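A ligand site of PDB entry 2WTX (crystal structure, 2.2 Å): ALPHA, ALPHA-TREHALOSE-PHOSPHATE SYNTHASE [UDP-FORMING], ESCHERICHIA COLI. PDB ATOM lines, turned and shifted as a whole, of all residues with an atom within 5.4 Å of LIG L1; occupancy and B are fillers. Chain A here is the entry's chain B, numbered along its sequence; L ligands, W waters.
OD2 of Asp 131 sits at hydrogen-bond distance from O7 of LIG L1, 2.5 Å away.
An oxygen (O3) of LIG L1 lies within hydrogen-bond range of the side-chain hydroxyl of Tyr 77 (2.6 Å).
A ring nitrogen (ND1) of His 155 sits at hydrogen-bond distance from an oxygen (O11) of LIG L1.
The side-chain carboxylate (OD1) of Asp 362 is in hydrogen-bond range of an oxygen (O9) of LIG L1.
O2 of LIG L1 lies within salt-bridge range of NE of Arg 10 (2.9 Å).
The backbone NH (N) of Asn 365 is in hydrogen-bond range of an oxygen (O10) of LIG L1, 2.9 Å away.
O9 of LIG L1 is in hydrogen-bond range of N of Met 364, at 3.0 Å.
NE of Arg 301 is in salt-bridge range of O3 of LIG L1.
N of Gly 363 lies within hydrogen-bond range of O9 of LIG L1.
The backbone carbonyl oxygen of Gly 23 is in hydrogen-bond range of an oxygen (O11) of LIG L1, at 3.2 Å.
The backbone NH of Leu 24 sits at hydrogen-bond distance from an oxygen (O11) of LIG L1.
N of Gly 23 sits at hydrogen-bond distance from O12 of LG2 L2, 2.6 Å away.
O7 of LG2 L2 lies within hydrogen-bond range of N of Leu 366 (2.9 Å).
An oxygen (O10) of LG2 L2 is in salt-bridge range of the guanidinium group (NE) of Arg 263 (2.8 Å).
O4 of LG2 L2 is in hydrogen-bond range of N of Gly 22.
An oxygen (O11) of LG2 L2 is in salt-bridge range of the side-chain amino group of Lys 268 (3.1 Å).
N1 of LIG L1 sits at hydrogen-bond distance from O12 of LG2 L2.
The backbone carbonyl oxygen (O) of Tyr 77 sits at hydrogen-bond distance from the backbone NH (N) of Asn 82, 2.9 Å away.
The backbone carbonyl oxygen of His 155 lies within hydrogen-bond range of the side-chain amide nitrogen of Gln 186, 3.0 Å away.
The side-chain carboxylate (OD2) of Asp 362 is in hydrogen-bond range of the side-chain amide nitrogen (ND2) of Asn 365.
The side-chain carboxylate (OD2) of Asp 362 is in salt-bridge range of the side-chain amino group (NZ) of Lys 268.
OH of Tyr 132 sits at hydrogen-bond distance from NH2 of Arg 301 (2.9 Å).
The backbone NH (N) of Ile 226 lies within hydrogen-bond range of the side-chain amide oxygen (OE1) of Gln 186 (3.2 Å).
A ring nitrogen (ND1) of His 90 is in hydrogen-bond range of the backbone carbonyl oxygen (O) of Trp 86 (2.9 Å).
The side-chain hydroxyl of Tyr 132 sits close to a ring nitrogen (NE2) of His 133, at 3.4 Å.
Ala 21 touches LIG L1.
Gly 22 touches LIG L1 (CA to C1, 3.7 Å).
Trp 86 touches LIG L1 (CH2 to O8, 3.5 Å).
CE1 of Tyr 132 touches O7 of LIG L1 (3.6 Å).
His 133 touches LIG L1.
Ile 156 touches LIG L1.
Ile 226 touches LIG L1.
Arg 263 touches LIG L1.
N of Leu 366 touches O10 of LIG L1, 3.5 Å away.
Within 4 Å of LIG L1: Arg 10, Ala 21, Gly 22, Gly 23, Leu 24, Tyr 77, Trp 86, Asp 131, Tyr 132, His 133, His 155, Ile 156, Ile 226, Arg 263, Arg 301, Asp 362, Gly 363, Met 364, Asn 365 and Leu 366.
The nearest printed residue that does not touch LIG L1 is Gln 186 (4.1 Å).
Water W4 lies within hydrogen-bond range of an oxygen (O5) of LIG L1 (2.7 Å) and the backbone NH (N) of Leu 24 (3.2 Å).
Water W3 lies within hydrogen-bond range of NE2 of His 133 (2.6 Å), O3 of LIG L1 (2.7 Å), OH of Tyr 132 (2.8 Å), OD1 of Asn 82 (2.9 Å) and NH2 of Arg 301 (3.2 Å).
Water W2 lies within hydrogen-bond range of a ring nitrogen (NE2) of His 90 (2.7 Å), the backbone NH of Gly 363 (2.8 Å), an oxygen (O8) of LIG L1 (2.8 Å) and the side-chain carboxylate of Asp 362 (3.4 Å).
Water W1 lies within hydrogen-bond range of an oxygen (O6) of LIG L1 (3.0 Å), the backbone NH of Arg 10 (3.1 Å) and a ring nitrogen (ND1) of His 133 (3.4 Å).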
ATOM      1  N   ARG A  10     -15.733  22.092  -2.025  1.00  0.00           N
ATOM      2  CA  ARG A  10     -14.719  21.557  -2.918  1.00  0.00           C
ATOM      3  C   ARG A  10     -13.896  22.699  -3.505  1.00  0.00           C
ATOM      4  O   ARG A  10     -14.457  23.660  -4.045  1.00  0.00           O
ATOM      5  CB  ARG A  10     -15.366  20.735  -4.037  1.00  0.00           C
ATOM      6  CG  ARG A  10     -14.387  20.018  -4.983  1.00  0.00           C
ATOM      7  CD  ARG A  10     -13.575  18.946  -4.240  1.00  0.00           C
ATOM      8  NE  ARG A  10     -14.357  17.736  -3.948  1.00  0.00           N
ATOM      9  CZ  ARG A  10     -13.951  16.779  -3.111  1.00  0.00           C
ATOM     10  NH1 ARG A  10     -12.796  16.895  -2.461  1.00  0.00           N
ATOM     11  NH2 ARG A  10     -14.724  15.717  -2.905  1.00  0.00           N
ATOM     12  N   SER A  20      -9.707  15.873  -9.143  1.00  0.00           N
ATOM     13  CA  SER A  20     -11.056  15.377  -8.826  1.00  0.00           C
ATOM     14  C   SER A  20     -12.133  15.886  -9.790  1.00  0.00           C
ATOM     15  O   SER A  20     -12.239  17.087 -10.025  1.00  0.00           O
ATOM     16  CB  SER A  20     -11.435  15.763  -7.382  1.00  0.00           C
ATOM     17  OG  SER A  20     -11.659  14.606  -6.586  1.00  0.00           O
ATOM     18  N   ALA A  21     -12.921  14.947 -10.333  1.00  0.00           N
ATOM     19  CA  ALA A  21     -14.094  15.256 -11.167  1.00  0.00           C
ATOM     20  C   ALA A  21     -15.139  16.130 -10.439  1.00  0.00           C
ATOM     21  O   ALA A  21     -15.390  15.927  -9.258  1.00  0.00           O
ATOM     22  CB  ALA A  21     -14.738  13.971 -11.657  1.00  0.00           C
ATOM     23  N   GLY A  22     -15.722  17.085 -11.172  1.00  0.00           N
ATOM     24  CA  GLY A  22     -16.692  18.059 -10.630  1.00  0.00           C
ATOM     25  C   GLY A  22     -16.596  19.425 -11.284  1.00  0.00           C
ATOM     26  O   GLY A  22     -15.492  19.989 -11.424  1.00  0.00           O
ATOM     27  N   GLY A  23     -17.736  19.992 -11.673  1.00  0.00           N
ATOM     28  CA  GLY A  23     -17.773  21.264 -12.398  1.00  0.00           C
ATOM     29  C   GLY A  23     -17.597  22.546 -11.598  1.00  0.00           C
ATOM     30  O   GLY A  23     -17.204  23.573 -12.173  1.00  0.00           O
ATOM     31  N   LEU A  24     -17.878  22.505 -10.300  1.00  0.00           N
ATOM     32  CA  LEU A  24     -17.779  23.697  -9.444  1.00  0.00           C
ATOM     33  C   LEU A  24     -16.337  24.215  -9.355  1.00  0.00           C
ATOM     34  O   LEU A  24     -16.081  25.397  -9.621  1.00  0.00           O
ATOM     35  CB  LEU A  24     -18.379  23.435  -8.056  1.00  0.00           C
ATOM     36  CG  LEU A  24     -18.161  24.474  -6.944  1.00  0.00           C
ATOM     37  CD1 LEU A  24     -19.343  24.563  -6.038  1.00  0.00           C
ATOM     38  CD2 LEU A  24     -16.903  24.142  -6.121  1.00  0.00           C
ATOM     39  N   GLY A  27     -15.084  25.642 -12.670  1.00  0.00           N
ATOM     40  CA  GLY A  27     -15.738  26.915 -12.952  1.00  0.00           C
ATOM     41  C   GLY A  27     -15.106  28.046 -12.166  1.00  0.00           C
ATOM     42  O   GLY A  27     -14.727  29.074 -12.727  1.00  0.00           O
ATOM     43  N   TYR A  77     -21.239  16.427   5.141  1.00  0.00           N
ATOM     44  CA  TYR A  77     -20.989  16.044   3.780  1.00  0.00           C
ATOM     45  C   TYR A  77     -21.763  14.786   3.313  1.00  0.00           C
ATOM     46  O   TYR A  77     -22.621  14.890   2.424  1.00  0.00           O
ATOM     47  CB  TYR A  77     -19.463  15.913   3.594  1.00  0.00           C
ATOM     48  CG  TYR A  77     -19.037  15.582   2.208  1.00  0.00           C
ATOM     49  CD1 TYR A  77     -18.964  16.585   1.211  1.00  0.00           C
ATOM     50  CD2 TYR A  77     -18.690  14.284   1.867  1.00  0.00           C
ATOM     51  CE1 TYR A  77     -18.566  16.264  -0.090  1.00  0.00           C
ATOM     52  CE2 TYR A  77     -18.281  13.953   0.592  1.00  0.00           C
ATOM     53  CZ  TYR A  77     -18.218  14.938  -0.385  1.00  0.00           C
ATOM     54  OH  TYR A  77     -17.825  14.559  -1.659  1.00  0.00           O
ATOM     55  N   ASN A  82     -24.991  15.288   0.871  1.00  0.00           N
ATOM     56  CA  ASN A  82     -25.021  14.271  -0.166  1.00  0.00           C
ATOM     57  C   ASN A  82     -26.145  13.270  -0.106  1.00  0.00           C
ATOM     58  O   ASN A  82     -26.393  12.586  -1.113  1.00  0.00           O
ATOM     59  CB  ASN A  82     -23.652  13.577  -0.307  1.00  0.00           C
ATOM     60  CG  ASN A  82     -22.581  14.545  -0.775  1.00  0.00           C
ATOM     61  OD1 ASN A  82     -22.898  15.605  -1.316  1.00  0.00           O
ATOM     62  ND2 ASN A  82     -21.317  14.204  -0.530  1.00  0.00           N
ATOM     63  N   TRP A  86     -28.611  16.877  -2.003  1.00  0.00           N
ATOM     64  CA  TRP A  86     -28.358  16.454  -3.389  1.00  0.00           C
ATOM     65  C   TRP A  86     -29.544  15.681  -3.987  1.00  0.00           C
ATOM     66  O   TRP A  86     -30.058  16.064  -5.043  1.00  0.00           O
ATOM     67  CB  TRP A  86     -27.014  15.689  -3.492  1.00  0.00           C
ATOM     68  CG  TRP A  86     -26.697  15.293  -4.913  1.00  0.00           C
ATOM     69  CD1 TRP A  86     -27.075  14.140  -5.555  1.00  0.00           C
ATOM     70  CD2 TRP A  86     -25.946  16.058  -5.879  1.00  0.00           C
ATOM     71  NE1 TRP A  86     -26.616  14.147  -6.842  1.00  0.00           N
ATOM     72  CE2 TRP A  86     -25.912  15.303  -7.067  1.00  0.00           C
ATOM     73  CE3 TRP A  86     -25.297  17.301  -5.837  1.00  0.00           C
ATOM     74  CZ2 TRP A  86     -25.238  15.742  -8.220  1.00  0.00           C
ATOM     75  CZ3 TRP A  86     -24.619  17.753  -6.986  1.00  0.00           C
ATOM     76  CH2 TRP A  86     -24.604  16.964  -8.164  1.00  0.00           C
ATOM     77  N   HIS A  90     -32.237  17.186  -6.901  1.00  0.00           N
ATOM     78  CA  HIS A  90     -32.275  16.468  -8.178  1.00  0.00           C
ATOM     79  C   HIS A  90     -33.524  15.624  -8.324  1.00  0.00           C
ATOM     80  O   HIS A  90     -33.517  14.612  -9.027  1.00  0.00           O
ATOM     81  CB  HIS A  90     -31.003  15.628  -8.379  1.00  0.00           C
ATOM     82  CG  HIS A  90     -29.791  16.459  -8.626  1.00  0.00           C
ATOM     83  ND1 HIS A  90     -29.084  17.068  -7.605  1.00  0.00           N
ATOM     84  CD2 HIS A  90     -29.187  16.859  -9.775  1.00  0.00           C
ATOM     85  CE1 HIS A  90     -28.082  17.763  -8.113  1.00  0.00           C
ATOM     86  NE2 HIS A  90     -28.121  17.655  -9.428  1.00  0.00           N
ATOM     87  N   ASP A 131     -22.530  27.131  -3.563  1.00  0.00           N
ATOM     88  CA  ASP A 131     -23.191  25.821  -3.599  1.00  0.00           C
ATOM     89  C   ASP A 131     -23.839  25.307  -2.302  1.00  0.00           C
ATOM     90  O   ASP A 131     -23.649  25.860  -1.217  1.00  0.00           O
ATOM     91  CB  ASP A 131     -22.276  24.766  -4.206  1.00  0.00           C
ATOM     92  CG  ASP A 131     -22.960  23.973  -5.306  1.00  0.00           C
ATOM     93  OD1 ASP A 131     -24.093  24.315  -5.718  1.00  0.00           O
ATOM     94  OD2 ASP A 131     -22.348  23.004  -5.797  1.00  0.00           O
ATOM     95  N   TYR A 132     -24.601  24.221  -2.467  1.00  0.00           N
ATOM     96  CA  TYR A 132     -25.563  23.708  -1.488  1.00  0.00           C
ATOM     97  C   TYR A 132     -24.978  23.335  -0.106  1.00  0.00           C
ATOM     98  O   TYR A 132     -25.725  23.310   0.878  1.00  0.00           O
ATOM     99  CB  TYR A 132     -26.362  22.542  -2.113  1.00  0.00           C
ATOM    100  CG  TYR A 132     -25.481  21.393  -2.549  1.00  0.00           C
ATOM    101  CD1 TYR A 132     -24.837  21.400  -3.792  1.00  0.00           C
ATOM    102  CD2 TYR A 132     -25.247  20.313  -1.708  1.00  0.00           C
ATOM    103  CE1 TYR A 132     -23.991  20.366  -4.184  1.00  0.00           C
ATOM    104  CE2 TYR A 132     -24.410  19.261  -2.080  1.00  0.00           C
ATOM    105  CZ  TYR A 132     -23.788  19.297  -3.318  1.00  0.00           C
ATOM    106  OH  TYR A 132     -22.968  18.250  -3.693  1.00  0.00           O
ATOM    107  N   HIS A 133     -23.679  23.083  -0.014  1.00  0.00           N
ATOM    108  CA  HIS A 133     -23.039  22.735   1.266  1.00  0.00           C
ATOM    109  C   HIS A 133     -23.100  23.892   2.246  1.00  0.00           C
ATOM    110  O   HIS A 133     -23.022  23.693   3.461  1.00  0.00           O
ATOM    111  CB  HIS A 133     -21.579  22.321   1.074  1.00  0.00           C
ATOM    112  CG  HIS A 133     -21.366  21.271   0.027  1.00  0.00           C
ATOM    113  ND1 HIS A 133     -21.271  21.571  -1.319  1.00  0.00           N
ATOM    114  CD2 HIS A 133     -21.228  19.925   0.133  1.00  0.00           C
ATOM    115  CE1 HIS A 133     -21.096  20.448  -2.001  1.00  0.00           C
ATOM    116  NE2 HIS A 133     -21.056  19.440  -1.146  1.00  0.00           N
ATOM    117  N   HIS A 155     -25.011  25.943  -7.825  1.00  0.00           N
ATOM    118  CA  HIS A 155     -24.551  25.263  -9.043  1.00  0.00           C
ATOM    119  C   HIS A 155     -25.506  24.183  -9.546  1.00  0.00           C
ATOM    120  O   HIS A 155     -25.401  23.724 -10.694  1.00  0.00           O
ATOM    121  CB  HIS A 155     -23.152  24.680  -8.817  1.00  0.00           C
ATOM    122  CG  HIS A 155     -22.066  25.720  -8.734  1.00  0.00           C
ATOM    123  ND1 HIS A 155     -21.252  26.028  -9.808  1.00  0.00           N
ATOM    124  CD2 HIS A 155     -21.677  26.533  -7.719  1.00  0.00           C
ATOM    125  CE1 HIS A 155     -20.411  26.982  -9.454  1.00  0.00           C
ATOM    126  NE2 HIS A 155     -20.642  27.302  -8.198  1.00  0.00           N
ATOM    127  N   ILE A 156     -26.443  23.777  -8.691  1.00  0.00           N
ATOM    128  CA  ILE A 156     -27.356  22.684  -9.009  1.00  0.00           C
ATOM    129  C   ILE A 156     -28.764  23.240  -9.242  1.00  0.00           C
ATOM    130  O   ILE A 156     -28.980  24.441  -9.005  1.00  0.00           O
ATOM    131  CB  ILE A 156     -27.322  21.601  -7.884  1.00  0.00           C
ATOM    132  CG1 ILE A 156     -27.799  22.174  -6.550  1.00  0.00           C
ATOM    133  CG2 ILE A 156     -25.906  21.022  -7.756  1.00  0.00           C
ATOM    134  CD1 ILE A 156     -27.863  21.107  -5.427  1.00  0.00           C
ATOM    135  N   GLN A 186     -28.468  28.912 -12.041  1.00  0.00           N
ATOM    136  CA  GLN A 186     -28.093  28.450 -13.385  1.00  0.00           C
ATOM    137  C   GLN A 186     -29.106  28.803 -14.474  1.00  0.00           C
ATOM    138  O   GLN A 186     -28.715  29.095 -15.604  1.00  0.00           O
ATOM    139  CB  GLN A 186     -27.835  26.931 -13.405  1.00  0.00           C
ATOM    140  CG  GLN A 186     -26.696  26.454 -12.494  1.00  0.00           C
ATOM    141  CD  GLN A 186     -25.315  26.605 -13.113  1.00  0.00           C
ATOM    142  OE1 GLN A 186     -25.080  27.457 -13.979  1.00  0.00           O
ATOM    143  NE2 GLN A 186     -24.381  25.773 -12.660  1.00  0.00           N
ATOM    144  N   ILE A 226     -23.264  29.185 -15.904  1.00  0.00           N
ATOM    145  CA  ILE A 226     -21.835  28.978 -15.912  1.00  0.00           C
ATOM    146  C   ILE A 226     -21.323  28.516 -17.303  1.00  0.00           C
ATOM    147  O   ILE A 226     -22.017  27.797 -18.048  1.00  0.00           O
ATOM    148  CB  ILE A 226     -21.398  28.008 -14.785  1.00  0.00           C
ATOM    149  CG1 ILE A 226     -19.896  28.166 -14.486  1.00  0.00           C
ATOM    150  CG2 ILE A 226     -21.801  26.558 -15.122  1.00  0.00           C
ATOM    151  CD1 ILE A 226     -19.456  27.584 -13.152  1.00  0.00           C
ATOM    152  N   ARG A 263     -19.108  11.875 -13.321  1.00  0.00           N
ATOM    153  CA  ARG A 263     -19.108  11.175 -12.041  1.00  0.00           C
ATOM    154  C   ARG A 263     -20.236  10.143 -12.067  1.00  0.00           C
ATOM    155  O   ARG A 263     -21.315  10.389 -12.647  1.00  0.00           O
ATOM    156  CB  ARG A 263     -19.321  12.135 -10.875  1.00  0.00           C
ATOM    157  CG  ARG A 263     -18.268  13.225 -10.714  1.00  0.00           C
ATOM    158  CD  ARG A 263     -18.654  14.147  -9.550  1.00  0.00           C
ATOM    159  NE  ARG A 263     -19.917  14.833  -9.872  1.00  0.00           N
ATOM    160  CZ  ARG A 263     -21.089  14.508  -9.358  1.00  0.00           C
ATOM    161  NH1 ARG A 263     -21.184  13.517  -8.470  1.00  0.00           N
ATOM    162  NH2 ARG A 263     -22.189  15.180  -9.728  1.00  0.00           N
ATOM    163  N   LYS A 268     -27.119  11.429 -13.299  1.00  0.00           N
ATOM    164  CA  LYS A 268     -26.600  11.360 -14.663  1.00  0.00           C
ATOM    165  C   LYS A 268     -27.276  10.345 -15.586  1.00  0.00           C
ATOM    166  O   LYS A 268     -26.915  10.250 -16.739  1.00  0.00           O
ATOM    167  CB  LYS A 268     -25.075  11.098 -14.656  1.00  0.00           C
ATOM    168  CG  LYS A 268     -24.253  12.077 -13.798  1.00  0.00           C
ATOM    169  CD  LYS A 268     -24.157  13.473 -14.424  1.00  0.00           C
ATOM    170  CE  LYS A 268     -23.423  14.439 -13.468  1.00  0.00           C
ATOM    171  NZ  LYS A 268     -23.028  15.718 -14.141  1.00  0.00           N
ATOM    172  N   SER A 300     -17.927   8.443  -7.295  1.00  0.00           N
ATOM    173  CA  SER A 300     -18.152   9.680  -6.556  1.00  0.00           C
ATOM    174  C   SER A 300     -18.947   9.333  -5.290  1.00  0.00           C
ATOM    175  O   SER A 300     -19.933   8.587  -5.361  1.00  0.00           O
ATOM    176  CB  SER A 300     -18.935  10.644  -7.449  1.00  0.00           C
ATOM    177  OG  SER A 300     -19.370  11.806  -6.761  1.00  0.00           O
ATOM    178  N   ARG A 301     -18.507   9.837  -4.135  1.00  0.00           N
ATOM    179  CA  ARG A 301     -19.293   9.785  -2.876  1.00  0.00           C
ATOM    180  C   ARG A 301     -19.652   8.340  -2.527  1.00  0.00           C
ATOM    181  O   ARG A 301     -20.784   8.040  -2.132  1.00  0.00           O
ATOM    182  CB  ARG A 301     -20.574  10.633  -2.998  1.00  0.00           C
ATOM    183  CG  ARG A 301     -20.320  12.097  -3.298  1.00  0.00           C
ATOM    184  CD  ARG A 301     -21.452  12.694  -4.151  1.00  0.00           C
ATOM    185  NE  ARG A 301     -21.141  14.058  -4.572  1.00  0.00           N
ATOM    186  CZ  ARG A 301     -22.046  14.967  -4.915  1.00  0.00           C
ATOM    187  NH1 ARG A 301     -23.346  14.654  -4.902  1.00  0.00           N
ATOM    188  NH2 ARG A 301     -21.657  16.182  -5.291  1.00  0.00           N
ATOM    189  N   ASP A 362     -29.471  18.145 -14.240  1.00  0.00           N
ATOM    190  CA  ASP A 362     -28.126  18.624 -14.089  1.00  0.00           C
ATOM    191  C   ASP A 362     -28.169  20.145 -13.980  1.00  0.00           C
ATOM    192  O   ASP A 362     -28.867  20.784 -14.710  1.00  0.00           O
ATOM    193  CB  ASP A 362     -27.266  18.128 -15.254  1.00  0.00           C
ATOM    194  CG  ASP A 362     -25.908  17.573 -14.815  1.00  0.00           C
ATOM    195  OD1 ASP A 362     -25.412  17.930 -13.751  1.00  0.00           O
ATOM    196  OD2 ASP A 362     -25.321  16.795 -15.556  1.00  0.00           O
ATOM    197  N   GLY A 363     -27.383  20.709 -13.091  1.00  0.00           N
ATOM    198  CA  GLY A 363     -27.394  22.125 -12.901  1.00  0.00           C
ATOM    199  C   GLY A 363     -27.042  22.846 -14.182  1.00  0.00           C
ATOM    200  O   GLY A 363     -27.728  23.751 -14.559  1.00  0.00           O
ATOM    201  N   MET A 364     -26.005  22.402 -14.858  1.00  0.00           N
ATOM    202  CA  MET A 364     -25.612  22.915 -16.143  1.00  0.00           C
ATOM    203  C   MET A 364     -25.077  21.802 -17.059  1.00  0.00           C
ATOM    204  O   MET A 364     -25.642  21.466 -18.066  1.00  0.00           O
ATOM    205  CB  MET A 364     -24.637  24.077 -15.994  1.00  0.00           C
ATOM    206  CG  MET A 364     -24.118  24.667 -17.284  1.00  0.00           C
ATOM    207  SD  MET A 364     -25.300  25.377 -18.407  1.00  0.00           S
ATOM    208  CE  MET A 364     -26.145  26.564 -17.439  1.00  0.00           C
ATOM    209  N   ASN A 365     -23.942  21.257 -16.632  1.00  0.00           N
ATOM    210  CA  ASN A 365     -23.182  20.222 -17.311  1.00  0.00           C
ATOM    211  C   ASN A 365     -22.098  20.847 -18.188  1.00  0.00           C
ATOM    212  O   ASN A 365     -22.320  21.162 -19.328  1.00  0.00           O
ATOM    213  CB  ASN A 365     -24.039  19.200 -18.075  1.00  0.00           C
ATOM    214  CG  ASN A 365     -23.263  17.932 -18.454  1.00  0.00           C
ATOM    215  OD1 ASN A 365     -22.389  17.970 -19.280  1.00  0.00           O
ATOM    216  ND2 ASN A 365     -23.596  16.824 -17.842  1.00  0.00           N
ATOM    217  N   LEU A 366     -20.940  21.026 -17.611  1.00  0.00           N
ATOM    218  CA  LEU A 366     -19.784  21.577 -18.282  1.00  0.00           C
ATOM    219  C   LEU A 366     -19.283  20.674 -19.387  1.00  0.00           C
ATOM    220  O   LEU A 366     -18.832  21.127 -20.382  1.00  0.00           O
ATOM    221  CB  LEU A 366     -18.669  21.931 -17.317  1.00  0.00           C
ATOM    222  CG  LEU A 366     -18.932  23.097 -16.370  1.00  0.00           C
ATOM    223  CD1 LEU A 366     -17.725  23.451 -15.640  1.00  0.00           C
ATOM    224  CD2 LEU A 366     -19.499  24.279 -17.057  1.00  0.00           C
HETATM  225  O1  LIG L   1     -16.789  15.245  -5.336  1.00  0.00           O
HETATM  226  P1  LIG L   1     -17.927  16.277  -4.940  1.00  0.00           P
HETATM  227  O2  LIG L   1     -17.168  17.654  -4.624  1.00  0.00           O
HETATM  228  O3  LIG L   1     -18.748  15.820  -3.750  1.00  0.00           O
HETATM  229  O4  LIG L   1     -18.781  16.514  -6.274  1.00  0.00           O
HETATM  230  C1  LIG L   1     -18.269  17.238  -7.422  1.00  0.00           C
HETATM  231  C2  LIG L   1     -19.115  18.484  -7.725  1.00  0.00           C
HETATM  232  C3  LIG L   1     -20.440  18.061  -8.400  1.00  0.00           C
HETATM  233  C4  LIG L   1     -19.326  19.290  -6.434  1.00  0.00           C
HETATM  234  O5  LIG L   1     -18.054  19.722  -5.914  1.00  0.00           O
HETATM  235  C5  LIG L   1     -20.244  20.491  -6.680  1.00  0.00           C
HETATM  236  O6  LIG L   1     -20.420  21.179  -5.446  1.00  0.00           O
HETATM  237  C6  LIG L   1     -21.599  20.011  -7.211  1.00  0.00           C
HETATM  238  O7  LIG L   1     -22.487  21.103  -7.419  1.00  0.00           O
HETATM  239  C7  LIG L   1     -21.472  19.215  -8.531  1.00  0.00           C
HETATM  240  N1  LIG L   1     -21.209  20.064  -9.752  1.00  0.00           N
HETATM  241  C8  LIG L   1     -22.276  21.039 -10.220  1.00  0.00           C
HETATM  242  C9  LIG L   1     -21.521  22.204 -10.878  1.00  0.00           C
HETATM  243  C10 LIG L   1     -23.409  20.480 -11.163  1.00  0.00           C
HETATM  244  O8  LIG L   1     -23.708  19.108 -10.843  1.00  0.00           O
HETATM  245  C11 LIG L   1     -23.140  20.613 -12.693  1.00  0.00           C
HETATM  246  O9  LIG L   1     -24.303  20.306 -13.481  1.00  0.00           O
HETATM  247  C12 LIG L   1     -22.752  22.021 -13.110  1.00  0.00           C
HETATM  248  O10 LIG L   1     -22.156  21.946 -14.425  1.00  0.00           O
HETATM  249  C13 LIG L   1     -21.702  22.612 -12.197  1.00  0.00           C
HETATM  250  C14 LIG L   1     -20.848  23.747 -12.766  1.00  0.00           C
HETATM  251  O11 LIG L   1     -20.276  24.486 -11.704  1.00  0.00           O
HETATM  252  N1  LG2 L   2     -13.873  15.448 -15.341  1.00  0.00           N
HETATM  253  C1  LG2 L   2     -12.521  15.171 -15.366  1.00  0.00           C
HETATM  254  N2  LG2 L   2     -12.075  13.863 -15.335  1.00  0.00           N
HETATM  255  C2  LG2 L   2     -12.980  12.811 -15.249  1.00  0.00           C
HETATM  256  C3  LG2 L   2     -14.351  13.081 -15.200  1.00  0.00           C
HETATM  257  C4  LG2 L   2     -14.770  14.413 -15.275  1.00  0.00           C
HETATM  258  O1  LG2 L   2     -11.705  16.090 -15.448  1.00  0.00           O
HETATM  259  O2  LG2 L   2     -12.567  11.659 -15.218  1.00  0.00           O
HETATM  260  C5  LG2 L   2     -14.313  16.871 -15.357  1.00  0.00           C
HETATM  261  C6  LG2 L   2     -14.994  17.352 -16.631  1.00  0.00           C
HETATM  262  O3  LG2 L   2     -14.104  17.745 -17.647  1.00  0.00           O
HETATM  263  C7  LG2 L   2     -15.840  18.516 -16.146  1.00  0.00           C
HETATM  264  C8  LG2 L   2     -16.162  18.150 -14.713  1.00  0.00           C
HETATM  265  O4  LG2 L   2     -15.244  17.145 -14.308  1.00  0.00           O
HETATM  266  O5  LG2 L   2     -15.101  19.726 -16.082  1.00  0.00           O
HETATM  267  C9  LG2 L   2     -17.608  17.680 -14.625  1.00  0.00           C
HETATM  268  O6  LG2 L   2     -18.442  18.819 -14.482  1.00  0.00           O
HETATM  269  P1  LG2 L   2     -19.974  18.727 -14.916  1.00  0.00           P
HETATM  270  O7  LG2 L   2     -20.564  20.088 -14.896  1.00  0.00           O
HETATM  271  O8  LG2 L   2     -20.142  18.057 -16.200  1.00  0.00           O
HETATM  272  O9  LG2 L   2     -20.743  17.739 -13.885  1.00  0.00           O
HETATM  273  P2  LG2 L   2     -20.551  17.642 -12.304  1.00  0.00           P
HETATM  274  O10 LG2 L   2     -19.585  16.580 -11.975  1.00  0.00           O
HETATM  275  O11 LG2 L   2     -21.894  17.305 -11.748  1.00  0.00           O
HETATM  276  O12 LG2 L   2     -20.101  18.889 -11.638  1.00  0.00           O
HETATM  277  O   HOH W   1     -18.545  21.988  -3.312  1.00  0.00           O
HETATM  278  O   HOH W   2     -26.516  19.325 -10.835  1.00  0.00           O
HETATM  279  O   HOH W   3     -20.732  17.196  -2.451  1.00  0.00           O
HETATM  280  O   HOH W   4     -16.612  20.579  -8.036  1.00  0.00           O
